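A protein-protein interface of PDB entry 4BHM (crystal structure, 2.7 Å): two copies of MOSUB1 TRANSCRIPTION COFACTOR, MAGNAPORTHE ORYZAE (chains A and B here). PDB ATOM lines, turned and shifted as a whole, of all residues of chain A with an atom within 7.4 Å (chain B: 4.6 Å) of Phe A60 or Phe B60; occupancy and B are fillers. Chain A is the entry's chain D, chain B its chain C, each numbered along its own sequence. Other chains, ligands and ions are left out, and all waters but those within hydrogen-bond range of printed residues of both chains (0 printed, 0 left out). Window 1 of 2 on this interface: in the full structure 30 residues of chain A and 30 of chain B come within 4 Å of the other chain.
The backbone NH (N) of Trp A12 sits at hydrogen-bond distance from the backbone carbonyl oxygen (O) of Val A20 (2.8 Å).
Among the printed residues, pairs that only touch across the chains: Trp A12 with Ala B63, Trp A12 with Ile B67, Ile A14 with Gln B56, Ile A14 with Ala B59, Ile A14 with Phe B60, Val A20 with Phe B60, Val A20 with Ile B67, Gln A56 with Ile B14, Tyr A57 with Ile B64, Tyr A57 with Ile B67, Ala A59 with Ile B14, Phe A60 with Ile B14, Phe A60 with Ile B33, Phe A60 with Phe B60, Leu A61 with Ile B64, Ile A64 with Tyr B57, Ile A64 with Leu B61, Ile A64 with Ile B64, Ile A67 with Val B20 and Ile A67 with Tyr B57.
Of the printed residues of chain B, Trp A12 touches Ala B63 and Ile B67. Of the printed residues of chain B, Ala A59 touches Ile B14 (3.7 Å). Printed residues of chain B within 4 Å of Ile A67: Val B20 (3.97 Å) and Tyr B57 (3.4 Å). Of the printed residues of chain A, Val B20 touches Ile A67. Of chain A, only Ile A14 comes within 4 Å of Ala B59. Phe B60 touches just these residues of chain A: Ile A14 (3.6 Å), Val A20 (3.6 Å) and Phe A60 (3.4 Å). Printed residues of chain A within 4 Å of Leu B61: Ile A64. The nearest printed residue of chain B that does not touch Phe A60 is Val B20 (4.1 Å).
Of the 13 printed residues of chain B, 11 touch a printed residue of chain A. Hydrophobic or aromatic side chains of chain B that line the printed part of chain A: Ile B14, Val B20, Ile B33, Tyr B57, Ala B59, Phe B60, Leu B61, Ala B63, Ile B64 and Ile B67. Of the 23 printed residues of chain A, 10 touch a printed residue of chain B. Printed residues of chain A that touch a printed residue of chain B: Trp A12, Ile A14, Val A20, Gln A56, Tyr A57, Ala A59, Phe A60, Leu A61, Ile A64 and Ile A67. Hydrophobic or aromatic side chains of chain A that line the printed part of chain B: Trp A12, Ile A14, Val A20, Tyr A57, Ala A59, Phe A60, Leu A61, Ile A64 and Ile A67. Among the printed residues, no Asp or Glu carboxylate lies within 4 Å of a Lys or Arg side-chain nitrogen of the other chain.
Ile A14 touches Ala B59, and with the chains exchanged Ala A59 touches Ile B14. Val A20 touches Ile B67, and with the chains exchanged Ile A67 touches Val B20. Tyr A57 touches Ile B64, and with the chains exchanged Ile A64 touches Tyr B57. Phe A60 touches Ile B33, but with the chains exchanged Ile A33 does not touch Phe B60 (4.1 Å). Positions printed for both chains: 14, 20, 33, 56, 57, 58, 59, 60, 61, 62, 63, 64 and 67.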
ATOM      1  N   TRP A  12     -23.476 -12.785  12.011  1.00  0.00           N
ATOM      2  CA  TRP A  12     -23.142 -12.822  10.592  1.00  0.00           C
ATOM      3  C   TRP A  12     -24.238 -13.600   9.856  1.00  0.00           C
ATOM      4  O   TRP A  12     -24.554 -14.732  10.214  1.00  0.00           O
ATOM      5  CB  TRP A  12     -21.748 -13.448  10.391  1.00  0.00           C
ATOM      6  CG  TRP A  12     -20.649 -12.627  10.997  1.00  0.00           C
ATOM      7  CD1 TRP A  12     -19.923 -11.656  10.377  1.00  0.00           C
ATOM      8  CD2 TRP A  12     -20.175 -12.674  12.354  1.00  0.00           C
ATOM      9  NE1 TRP A  12     -19.020 -11.098  11.256  1.00  0.00           N
ATOM     10  CE2 TRP A  12     -19.158 -11.702  12.477  1.00  0.00           C
ATOM     11  CE3 TRP A  12     -20.517 -13.434  13.475  1.00  0.00           C
ATOM     12  CZ2 TRP A  12     -18.475 -11.478  13.672  1.00  0.00           C
ATOM     13  CZ3 TRP A  12     -19.832 -13.215  14.655  1.00  0.00           C
ATOM     14  CH2 TRP A  12     -18.822 -12.246  14.745  1.00  0.00           C
ATOM     15  N   GLU A  13     -24.861 -12.979   8.865  1.00  0.00           N
ATOM     16  CA  GLU A  13     -25.929 -13.653   8.120  1.00  0.00           C
ATOM     17  C   GLU A  13     -25.362 -14.743   7.226  1.00  0.00           C
ATOM     18  O   GLU A  13     -24.414 -14.523   6.475  1.00  0.00           O
ATOM     19  CB  GLU A  13     -26.728 -12.670   7.251  1.00  0.00           C
ATOM     20  CG  GLU A  13     -27.477 -11.584   8.017  1.00  0.00           C
ATOM     21  CD  GLU A  13     -28.921 -11.954   8.364  1.00  0.00           C
ATOM     22  OE1 GLU A  13     -29.317 -13.140   8.206  1.00  0.00           O
ATOM     23  OE2 GLU A  13     -29.662 -11.039   8.800  1.00  0.00           O
ATOM     24  N   ILE A  14     -25.950 -15.926   7.296  1.00  0.00           N
ATOM     25  CA  ILE A  14     -25.585 -16.964   6.343  1.00  0.00           C
ATOM     26  C   ILE A  14     -26.746 -17.309   5.386  1.00  0.00           C
ATOM     27  O   ILE A  14     -26.618 -18.185   4.543  1.00  0.00           O
ATOM     28  CB  ILE A  14     -24.962 -18.200   7.040  1.00  0.00           C
ATOM     29  CG1 ILE A  14     -25.947 -18.852   7.994  1.00  0.00           C
ATOM     30  CG2 ILE A  14     -23.661 -17.814   7.800  1.00  0.00           C
ATOM     31  CD1 ILE A  14     -25.425 -20.151   8.539  1.00  0.00           C
ATOM     32  N   ARG A  19     -28.439 -17.206  10.770  1.00  0.00           N
ATOM     33  CA  ARG A  19     -27.386 -16.406  11.417  1.00  0.00           C
ATOM     34  C   ARG A  19     -26.345 -17.227  12.165  1.00  0.00           C
ATOM     35  O   ARG A  19     -26.658 -18.245  12.777  1.00  0.00           O
ATOM     36  CB  ARG A  19     -27.989 -15.477  12.466  1.00  0.00           C
ATOM     37  CG  ARG A  19     -28.721 -14.289  11.942  1.00  0.00           C
ATOM     38  CD  ARG A  19     -29.347 -13.503  13.080  1.00  0.00           C
ATOM     39  NE  ARG A  19     -30.150 -12.394  12.580  1.00  0.00           N
ATOM     40  CZ  ARG A  19     -30.623 -11.413  13.336  1.00  0.00           C
ATOM     41  NH1 ARG A  19     -30.365 -11.401  14.638  1.00  0.00           N
ATOM     42  NH2 ARG A  19     -31.347 -10.447  12.785  1.00  0.00           N
ATOM     43  N   VAL A  20     -25.105 -16.758  12.154  1.00  0.00           N
ATOM     44  CA  VAL A  20     -24.153 -17.240  13.138  1.00  0.00           C
ATOM     45  C   VAL A  20     -23.871 -16.129  14.114  1.00  0.00           C
ATOM     46  O   VAL A  20     -23.625 -15.005  13.709  1.00  0.00           O
ATOM     47  CB  VAL A  20     -22.850 -17.682  12.520  1.00  0.00           C
ATOM     48  CG1 VAL A  20     -22.003 -18.343  13.581  1.00  0.00           C
ATOM     49  CG2 VAL A  20     -23.136 -18.656  11.424  1.00  0.00           C
ATOM     50  N   GLY A  21     -23.926 -16.440  15.401  1.00  0.00           N
ATOM     51  CA  GLY A  21     -23.650 -15.448  16.425  1.00  0.00           C
ATOM     52  C   GLY A  21     -22.851 -15.969  17.598  1.00  0.00           C
ATOM     53  O   GLY A  21     -22.646 -17.166  17.760  1.00  0.00           O
ATOM     54  N   ILE A  31     -21.649 -20.286  20.623  1.00  0.00           N
ATOM     55  CA  ILE A  31     -21.658 -19.945  19.219  1.00  0.00           C
ATOM     56  C   ILE A  31     -22.953 -20.502  18.671  1.00  0.00           C
ATOM     57  O   ILE A  31     -23.138 -21.707  18.628  1.00  0.00           O
ATOM     58  CB  ILE A  31     -20.449 -20.539  18.462  1.00  0.00           C
ATOM     59  CG1 ILE A  31     -19.125 -19.929  18.956  1.00  0.00           C
ATOM     60  CG2 ILE A  31     -20.580 -20.239  16.980  1.00  0.00           C
ATOM     61  CD1 ILE A  31     -18.659 -20.324  20.372  1.00  0.00           C
ATOM     62  N   ASN A  32     -23.869 -19.624  18.293  1.00  0.00           N
ATOM     63  CA  ASN A  32     -25.173 -20.077  17.832  1.00  0.00           C
ATOM     64  C   ASN A  32     -25.316 -20.056  16.335  1.00  0.00           C
ATOM     65  O   ASN A  32     -24.960 -19.079  15.679  1.00  0.00           O
ATOM     66  CB  ASN A  32     -26.285 -19.240  18.440  1.00  0.00           C
ATOM     67  CG  ASN A  32     -26.399 -19.451  19.909  1.00  0.00           C
ATOM     68  OD1 ASN A  32     -25.827 -18.696  20.695  1.00  0.00           O
ATOM     69  ND2 ASN A  32     -27.117 -20.503  20.304  1.00  0.00           N
ATOM     70  N   ILE A  33     -25.837 -21.149  15.803  1.00  0.00           N
ATOM     71  CA  ILE A  33     -26.201 -21.236  14.405  1.00  0.00           C
ATOM     72  C   ILE A  33     -27.691 -21.516  14.415  1.00  0.00           C
ATOM     73  O   ILE A  33     -28.117 -22.535  14.919  1.00  0.00           O
ATOM     74  CB  ILE A  33     -25.376 -22.332  13.743  1.00  0.00           C
ATOM     75  CG1 ILE A  33     -23.893 -21.945  13.855  1.00  0.00           C
ATOM     76  CG2 ILE A  33     -25.766 -22.510  12.291  1.00  0.00           C
ATOM     77  CD1 ILE A  33     -22.931 -23.091  13.806  1.00  0.00           C
ATOM     78  N   LEU A  52     -23.622 -23.881  20.372  1.00  0.00           N
ATOM     79  CA  LEU A  52     -22.390 -24.619  20.553  1.00  0.00           C
ATOM     80  C   LEU A  52     -21.582 -24.014  21.673  1.00  0.00           C
ATOM     81  O   LEU A  52     -21.502 -22.793  21.813  1.00  0.00           O
ATOM     82  CB  LEU A  52     -21.570 -24.614  19.261  1.00  0.00           C
ATOM     83  CG  LEU A  52     -22.046 -25.468  18.080  1.00  0.00           C
ATOM     84  CD1 LEU A  52     -21.024 -25.417  16.940  1.00  0.00           C
ATOM     85  CD2 LEU A  52     -22.328 -26.930  18.486  1.00  0.00           C
ATOM     86  N   VAL A  54     -17.826 -23.438  23.392  1.00  0.00           N
ATOM     87  CA  VAL A  54     -16.522 -23.140  22.822  1.00  0.00           C
ATOM     88  C   VAL A  54     -15.746 -24.414  22.469  1.00  0.00           C
ATOM     89  O   VAL A  54     -15.249 -24.548  21.343  1.00  0.00           O
ATOM     90  CB  VAL A  54     -15.699 -22.217  23.763  1.00  0.00           C
ATOM     91  CG1 VAL A  54     -14.293 -22.027  23.241  1.00  0.00           C
ATOM     92  CG2 VAL A  54     -16.387 -20.875  23.904  1.00  0.00           C
ATOM     93  N   ASP A  55     -15.666 -25.343  23.426  1.00  0.00           N
ATOM     94  CA  ASP A  55     -15.034 -26.647  23.204  1.00  0.00           C
ATOM     95  C   ASP A  55     -15.609 -27.363  21.993  1.00  0.00           C
ATOM     96  O   ASP A  55     -14.877 -27.974  21.212  1.00  0.00           O
ATOM     97  CB  ASP A  55     -15.184 -27.550  24.425  1.00  0.00           C
ATOM     98  CG  ASP A  55     -14.736 -26.873  25.707  1.00  0.00           C
ATOM     99  OD1 ASP A  55     -15.283 -25.789  26.016  1.00  0.00           O
ATOM    100  OD2 ASP A  55     -13.838 -27.412  26.396  1.00  0.00           O
ATOM    101  N   GLN A  56     -16.927 -27.284  21.851  1.00  0.00           N
ATOM    102  CA  GLN A  56     -17.608 -27.874  20.714  1.00  0.00           C
ATOM    103  C   GLN A  56     -17.255 -27.149  19.408  1.00  0.00           C
ATOM    104  O   GLN A  56     -16.983 -27.786  18.387  1.00  0.00           O
ATOM    105  CB  GLN A  56     -19.121 -27.867  20.944  1.00  0.00           C
ATOM    106  CG  GLN A  56     -19.648 -28.973  21.852  1.00  0.00           C
ATOM    107  CD  GLN A  56     -20.993 -28.616  22.443  1.00  0.00           C
ATOM    108  OE1 GLN A  56     -21.576 -27.578  22.089  1.00  0.00           O
ATOM    109  NE2 GLN A  56     -21.489 -29.449  23.361  1.00  0.00           N
ATOM    110  N   TYR A  57     -17.260 -25.818  19.440  1.00  0.00           N
ATOM    111  CA  TYR A  57     -16.903 -25.040  18.266  1.00  0.00           C
ATOM    112  C   TYR A  57     -15.454 -25.266  17.853  1.00  0.00           C
ATOM    113  O   TYR A  57     -15.124 -25.211  16.668  1.00  0.00           O
ATOM    114  CB  TYR A  57     -17.185 -23.560  18.496  1.00  0.00           C
ATOM    115  CG  TYR A  57     -16.648 -22.621  17.425  1.00  0.00           C
ATOM    116  CD1 TYR A  57     -17.363 -22.375  16.256  1.00  0.00           C
ATOM    117  CD2 TYR A  57     -15.436 -21.968  17.591  1.00  0.00           C
ATOM    118  CE1 TYR A  57     -16.876 -21.510  15.286  1.00  0.00           C
ATOM    119  CE2 TYR A  57     -14.949 -21.107  16.629  1.00  0.00           C
ATOM    120  CZ  TYR A  57     -15.670 -20.883  15.479  1.00  0.00           C
ATOM    121  OH  TYR A  57     -15.175 -20.025  14.522  1.00  0.00           O
ATOM    122  N   THR A  58     -14.575 -25.530  18.811  1.00  0.00           N
ATOM    123  CA  THR A  58     -13.190 -25.817  18.426  1.00  0.00           C
ATOM    124  C   THR A  58     -13.016 -27.236  17.864  1.00  0.00           C
ATOM    125  O   THR A  58     -12.193 -27.463  16.971  1.00  0.00           O
ATOM    126  CB  THR A  58     -12.171 -25.548  19.549  1.00  0.00           C
ATOM    127  OG1 THR A  58     -12.386 -26.464  20.620  1.00  0.00           O
ATOM    128  CG2 THR A  58     -12.305 -24.131  20.049  1.00  0.00           C
ATOM    129  N   ALA A  59     -13.779 -28.187  18.391  1.00  0.00           N
ATOM    130  CA  ALA A  59     -13.774 -29.522  17.817  1.00  0.00           C
ATOM    131  C   ALA A  59     -14.242 -29.445  16.344  1.00  0.00           C
ATOM    132  O   ALA A  59     -13.588 -29.965  15.441  1.00  0.00           O
ATOM    133  CB  ALA A  59     -14.647 -30.473  18.645  1.00  0.00           C
ATOM    134  N   PHE A  60     -15.362 -28.774  16.123  1.00  0.00           N
ATOM    135  CA  PHE A  60     -15.812 -28.458  14.785  1.00  0.00           C
ATOM    136  C   PHE A  60     -14.655 -27.950  13.917  1.00  0.00           C
ATOM    137  O   PHE A  60     -14.387 -28.527  12.858  1.00  0.00           O
ATOM    138  CB  PHE A  60     -16.943 -27.428  14.852  1.00  0.00           C
ATOM    139  CG  PHE A  60     -17.695 -27.244  13.566  1.00  0.00           C
ATOM    140  CD1 PHE A  60     -17.265 -27.825  12.389  1.00  0.00           C
ATOM    141  CD2 PHE A  60     -18.843 -26.477  13.539  1.00  0.00           C
ATOM    142  CE1 PHE A  60     -17.957 -27.637  11.220  1.00  0.00           C
ATOM    143  CE2 PHE A  60     -19.547 -26.290  12.367  1.00  0.00           C
ATOM    144  CZ  PHE A  60     -19.103 -26.869  11.211  1.00  0.00           C
ATOM    145  N   LEU A  61     -13.979 -26.887  14.364  1.00  0.00           N
ATOM    146  CA  LEU A  61     -12.934 -26.237  13.580  1.00  0.00           C
ATOM    147  C   LEU A  61     -11.839 -27.193  13.136  1.00  0.00           C
ATOM    148  O   LEU A  61     -11.230 -26.995  12.085  1.00  0.00           O
ATOM    149  CB  LEU A  61     -12.276 -25.111  14.369  1.00  0.00           C
ATOM    150  CG  LEU A  61     -12.976 -23.783  14.644  1.00  0.00           C
ATOM    151  CD1 LEU A  61     -12.019 -22.880  15.402  1.00  0.00           C
ATOM    152  CD2 LEU A  61     -13.457 -23.138  13.355  1.00  0.00           C
ATOM    153  N   LYS A  62     -11.577 -28.217  13.936  1.00  0.00           N
ATOM    154  CA  LYS A  62     -10.476 -29.129  13.638  1.00  0.00           C
ATOM    155  C   LYS A  62     -10.924 -30.131  12.581  1.00  0.00           C
ATOM    156  O   LYS A  62     -10.107 -30.730  11.884  1.00  0.00           O
ATOM    157  CB  LYS A  62      -9.967 -29.832  14.919  1.00  0.00           C
ATOM    158  N   ALA A  63     -12.236 -30.284  12.453  1.00  0.00           N
ATOM    159  CA  ALA A  63     -12.822 -31.221  11.503  1.00  0.00           C
ATOM    160  C   ALA A  63     -12.990 -30.597  10.116  1.00  0.00           C
ATOM    161  O   ALA A  63     -13.147 -31.307   9.118  1.00  0.00           O
ATOM    162  CB  ALA A  63     -14.157 -31.714  12.023  1.00  0.00           C
ATOM    163  N   ILE A  64     -12.943 -29.269  10.069  1.00  0.00           N
ATOM    164  CA  ILE A  64     -13.232 -28.504   8.853  1.00  0.00           C
ATOM    165  C   ILE A  64     -12.413 -28.826   7.583  1.00  0.00           C
ATOM    166  O   ILE A  64     -12.972 -28.898   6.486  1.00  0.00           O
ATOM    167  CB  ILE A  64     -13.250 -26.988   9.151  1.00  0.00           C
ATOM    168  CG1 ILE A  64     -14.629 -26.602   9.686  1.00  0.00           C
ATOM    169  CG2 ILE A  64     -12.919 -26.183   7.923  1.00  0.00           C
ATOM    170  CD1 ILE A  64     -14.657 -25.282  10.374  1.00  0.00           C
ATOM    171  N   PRO A  65     -11.099 -29.043   7.720  1.00  0.00           N
ATOM    172  CA  PRO A  65     -10.379 -29.314   6.475  1.00  0.00           C
ATOM    173  C   PRO A  65     -10.860 -30.591   5.820  1.00  0.00           C
ATOM    174  O   PRO A  65     -10.942 -30.635   4.601  1.00  0.00           O
ATOM    175  CB  PRO A  65      -8.925 -29.478   6.932  1.00  0.00           C
ATOM    176  CG  PRO A  65      -8.863 -28.860   8.261  1.00  0.00           C
ATOM    177  CD  PRO A  65     -10.203 -29.044   8.882  1.00  0.00           C
ATOM    178  N   ILE A  67     -13.914 -32.110   6.247  1.00  0.00           N
ATOM    179  CA  ILE A  67     -15.254 -31.834   5.756  1.00  0.00           C
ATOM    180  C   ILE A  67     -15.190 -31.210   4.358  1.00  0.00           C
ATOM    181  O   ILE A  67     -15.846 -31.675   3.425  1.00  0.00           O
ATOM    182  CB  ILE A  67     -15.999 -30.893   6.702  1.00  0.00           C
ATOM    183  CG1 ILE A  67     -16.283 -31.588   8.023  1.00  0.00           C
ATOM    184  CG2 ILE A  67     -17.315 -30.443   6.105  1.00  0.00           C
ATOM    185  CD1 ILE A  67     -17.025 -30.685   8.971  1.00  0.00           C
ATOM    186  N   ILE B  14     -18.172 -33.860  17.747  1.00  0.00           N
ATOM    187  CA  ILE B  14     -17.653 -32.655  18.376  1.00  0.00           C
ATOM    188  C   ILE B  14     -18.054 -32.621  19.843  1.00  0.00           C
ATOM    189  O   ILE B  14     -17.974 -31.584  20.487  1.00  0.00           O
ATOM    190  CB  ILE B  14     -18.132 -31.370  17.668  1.00  0.00           C
ATOM    191  CG1 ILE B  14     -19.644 -31.208  17.784  1.00  0.00           C
ATOM    192  CG2 ILE B  14     -17.679 -31.339  16.188  1.00  0.00           C
ATOM    193  CD1 ILE B  14     -20.157 -30.026  16.994  1.00  0.00           C
ATOM    194  N   VAL B  20     -21.072 -33.400  13.479  1.00  0.00           N
ATOM    195  CA  VAL B  20     -21.258 -32.780  12.173  1.00  0.00           C
ATOM    196  C   VAL B  20     -21.193 -33.890  11.142  1.00  0.00           C
ATOM    197  O   VAL B  20     -20.337 -34.762  11.206  1.00  0.00           O
ATOM    198  CB  VAL B  20     -20.207 -31.691  11.861  1.00  0.00           C
ATOM    199  CG1 VAL B  20     -20.621 -30.914  10.633  1.00  0.00           C
ATOM    200  CG2 VAL B  20     -20.100 -30.730  13.002  1.00  0.00           C
ATOM    201  N   ILE B  33     -25.516 -30.283  11.863  1.00  0.00           N
ATOM    202  CA  ILE B  33     -24.892 -30.048  13.150  1.00  0.00           C
ATOM    203  C   ILE B  33     -26.043 -30.299  14.106  1.00  0.00           C
ATOM    204  O   ILE B  33     -27.046 -29.573  14.099  1.00  0.00           O
ATOM    205  CB  ILE B  33     -24.348 -28.617  13.242  1.00  0.00           C
ATOM    206  CG1 ILE B  33     -23.476 -28.314  12.024  1.00  0.00           C
ATOM    207  CG2 ILE B  33     -23.523 -28.430  14.502  1.00  0.00           C
ATOM    208  CD1 ILE B  33     -23.432 -26.861  11.645  1.00  0.00           C
ATOM    209  N   GLN B  56     -24.821 -22.120   2.671  1.00  0.00           N
ATOM    210  CA  GLN B  56     -24.933 -21.625   4.025  1.00  0.00           C
ATOM    211  C   GLN B  56     -23.695 -22.007   4.847  1.00  0.00           C
ATOM    212  O   GLN B  56     -23.298 -21.282   5.745  1.00  0.00           O
ATOM    213  CB  GLN B  56     -26.192 -22.183   4.675  1.00  0.00           C
ATOM    214  CG  GLN B  56     -27.463 -21.583   4.145  1.00  0.00           C
ATOM    215  CD  GLN B  56     -28.694 -22.332   4.614  1.00  0.00           C
ATOM    216  OE1 GLN B  56     -28.596 -23.365   5.292  1.00  0.00           O
ATOM    217  NE2 GLN B  56     -29.867 -21.821   4.246  1.00  0.00           N
ATOM    218  N   TYR B  57     -23.092 -23.147   4.528  1.00  0.00           N
ATOM    219  CA  TYR B  57     -21.897 -23.590   5.211  1.00  0.00           C
ATOM    220  C   TYR B  57     -20.683 -22.802   4.715  1.00  0.00           C
ATOM    221  O   TYR B  57     -19.734 -22.547   5.483  1.00  0.00           O
ATOM    222  CB  TYR B  57     -21.706 -25.086   4.997  1.00  0.00           C
ATOM    223  CG  TYR B  57     -20.354 -25.610   5.391  1.00  0.00           C
ATOM    224  CD1 TYR B  57     -20.040 -25.859   6.723  1.00  0.00           C
ATOM    225  CD2 TYR B  57     -19.390 -25.893   4.422  1.00  0.00           C
ATOM    226  CE1 TYR B  57     -18.783 -26.351   7.084  1.00  0.00           C
ATOM    227  CE2 TYR B  57     -18.143 -26.393   4.767  1.00  0.00           C
ATOM    228  CZ  TYR B  57     -17.841 -26.608   6.102  1.00  0.00           C
ATOM    229  OH  TYR B  57     -16.598 -27.091   6.435  1.00  0.00           O
ATOM    230  N   THR B  58     -20.700 -22.391   3.449  1.00  0.00           N
ATOM    231  CA  THR B  58     -19.561 -21.636   2.967  1.00  0.00           C
ATOM    232  C   THR B  58     -19.611 -20.173   3.396  1.00  0.00           C
ATOM    233  O   THR B  58     -18.567 -19.532   3.496  1.00  0.00           O
ATOM    234  CB  THR B  58     -19.317 -21.774   1.453  1.00  0.00           C
ATOM    235  OG1 THR B  58     -20.423 -21.243   0.717  1.00  0.00           O
ATOM    236  CG2 THR B  58     -19.081 -23.211   1.084  1.00  0.00           C
ATOM    237  N   ALA B  59     -20.812 -19.650   3.639  1.00  0.00           N
ATOM    238  CA  ALA B  59     -20.961 -18.329   4.245  1.00  0.00           C
ATOM    239  C   ALA B  59     -20.430 -18.411   5.677  1.00  0.00           C
ATOM    240  O   ALA B  59     -19.690 -17.528   6.148  1.00  0.00           O
ATOM    241  CB  ALA B  59     -22.404 -17.902   4.246  1.00  0.00           C
ATOM    242  N   PHE B  60     -20.809 -19.493   6.348  1.00  0.00           N
ATOM    243  CA  PHE B  60     -20.289 -19.816   7.656  1.00  0.00           C
ATOM    244  C   PHE B  60     -18.760 -19.850   7.728  1.00  0.00           C
ATOM    245  O   PHE B  60     -18.183 -19.336   8.680  1.00  0.00           O
ATOM    246  CB  PHE B  60     -20.862 -21.148   8.111  1.00  0.00           C
ATOM    247  CG  PHE B  60     -20.335 -21.611   9.419  1.00  0.00           C
ATOM    248  CD1 PHE B  60     -20.387 -20.787  10.528  1.00  0.00           C
ATOM    249  CD2 PHE B  60     -19.794 -22.878   9.552  1.00  0.00           C
ATOM    250  CE1 PHE B  60     -19.897 -21.221  11.772  1.00  0.00           C
ATOM    251  CE2 PHE B  60     -19.303 -23.323  10.783  1.00  0.00           C
ATOM    252  CZ  PHE B  60     -19.356 -22.493  11.897  1.00  0.00           C
ATOM    253  N   LEU B  61     -18.105 -20.450   6.740  1.00  0.00           N
ATOM    254  CA  LEU B  61     -16.646 -20.595   6.775  1.00  0.00           C
ATOM    255  C   LEU B  61     -15.914 -19.263   6.701  1.00  0.00           C
ATOM    256  O   LEU B  61     -14.724 -19.178   6.991  1.00  0.00           O
ATOM    257  CB  LEU B  61     -16.155 -21.474   5.622  1.00  0.00           C
ATOM    258  CG  LEU B  61     -16.454 -22.972   5.617  1.00  0.00           C
ATOM    259  CD1 LEU B  61     -16.039 -23.535   4.274  1.00  0.00           C
ATOM    260  CD2 LEU B  61     -15.752 -23.706   6.765  1.00  0.00           C
ATOM    261  N   LYS B  62     -16.634 -18.231   6.287  1.00  0.00           N
ATOM    262  CA  LYS B  62     -16.043 -16.944   6.013  1.00  0.00           C
ATOM    263  C   LYS B  62     -16.216 -16.038   7.213  1.00  0.00           C
ATOM    264  O   LYS B  62     -15.485 -15.053   7.373  1.00  0.00           O
ATOM    265  CB  LYS B  62     -16.706 -16.320   4.786  1.00  0.00           C
ATOM    266  CG  LYS B  62     -16.323 -16.946   3.453  1.00  0.00           C
ATOM    267  CD  LYS B  62     -17.179 -16.362   2.329  1.00  0.00           C
ATOM    268  CE  LYS B  62     -16.580 -16.610   0.949  1.00  0.00           C
ATOM    269  NZ  LYS B  62     -16.827 -15.458   0.017  1.00  0.00           N
ATOM    270  N   ALA B  63     -17.187 -16.360   8.060  1.00  0.00           N
ATOM    271  CA  ALA B  63     -17.387 -15.595   9.276  1.00  0.00           C
ATOM    272  C   ALA B  63     -16.487 -16.144  10.387  1.00  0.00           C
ATOM    273  O   ALA B  63     -16.300 -15.502  11.431  1.00  0.00           O
ATOM    274  CB  ALA B  63     -18.834 -15.591   9.687  1.00  0.00           C
ATOM    275  N   ILE B  64     -15.902 -17.312  10.144  1.00  0.00           N
ATOM    276  CA  ILE B  64     -15.036 -17.953  11.134  1.00  0.00           C
ATOM    277  C   ILE B  64     -13.841 -17.123  11.645  1.00  0.00           C
ATOM    278  O   ILE B  64     -13.566 -17.119  12.847  1.00  0.00           O
ATOM    279  CB  ILE B  64     -14.600 -19.377  10.689  1.00  0.00           C
ATOM    280  CG1 ILE B  64     -15.787 -20.352  10.808  1.00  0.00           C
ATOM    281  CG2 ILE B  64     -13.395 -19.867  11.500  1.00  0.00           C
ATOM    282  CD1 ILE B  64     -15.467 -21.791  10.408  1.00  0.00           C
ATOM    283  N   ILE B  67     -15.328 -14.641  14.130  1.00  0.00           N
ATOM    284  CA  ILE B  67     -15.755 -15.359  15.331  1.00  0.00           C
ATOM    285  C   ILE B  67     -14.559 -15.747  16.207  1.00  0.00           C
ATOM    286  O   ILE B  67     -14.573 -15.560  17.433  1.00  0.00           O
ATOM    287  CB  ILE B  67     -16.529 -16.646  14.962  1.00  0.00           C
ATOM    288  CG1 ILE B  67     -17.903 -16.297  14.408  1.00  0.00           C
ATOM    289  CG2 ILE B  67     -16.671 -17.567  16.176  1.00  0.00           C
ATOM    290  CD1 ILE B  67     -18.484 -17.381  13.556  1.00  0.00           C
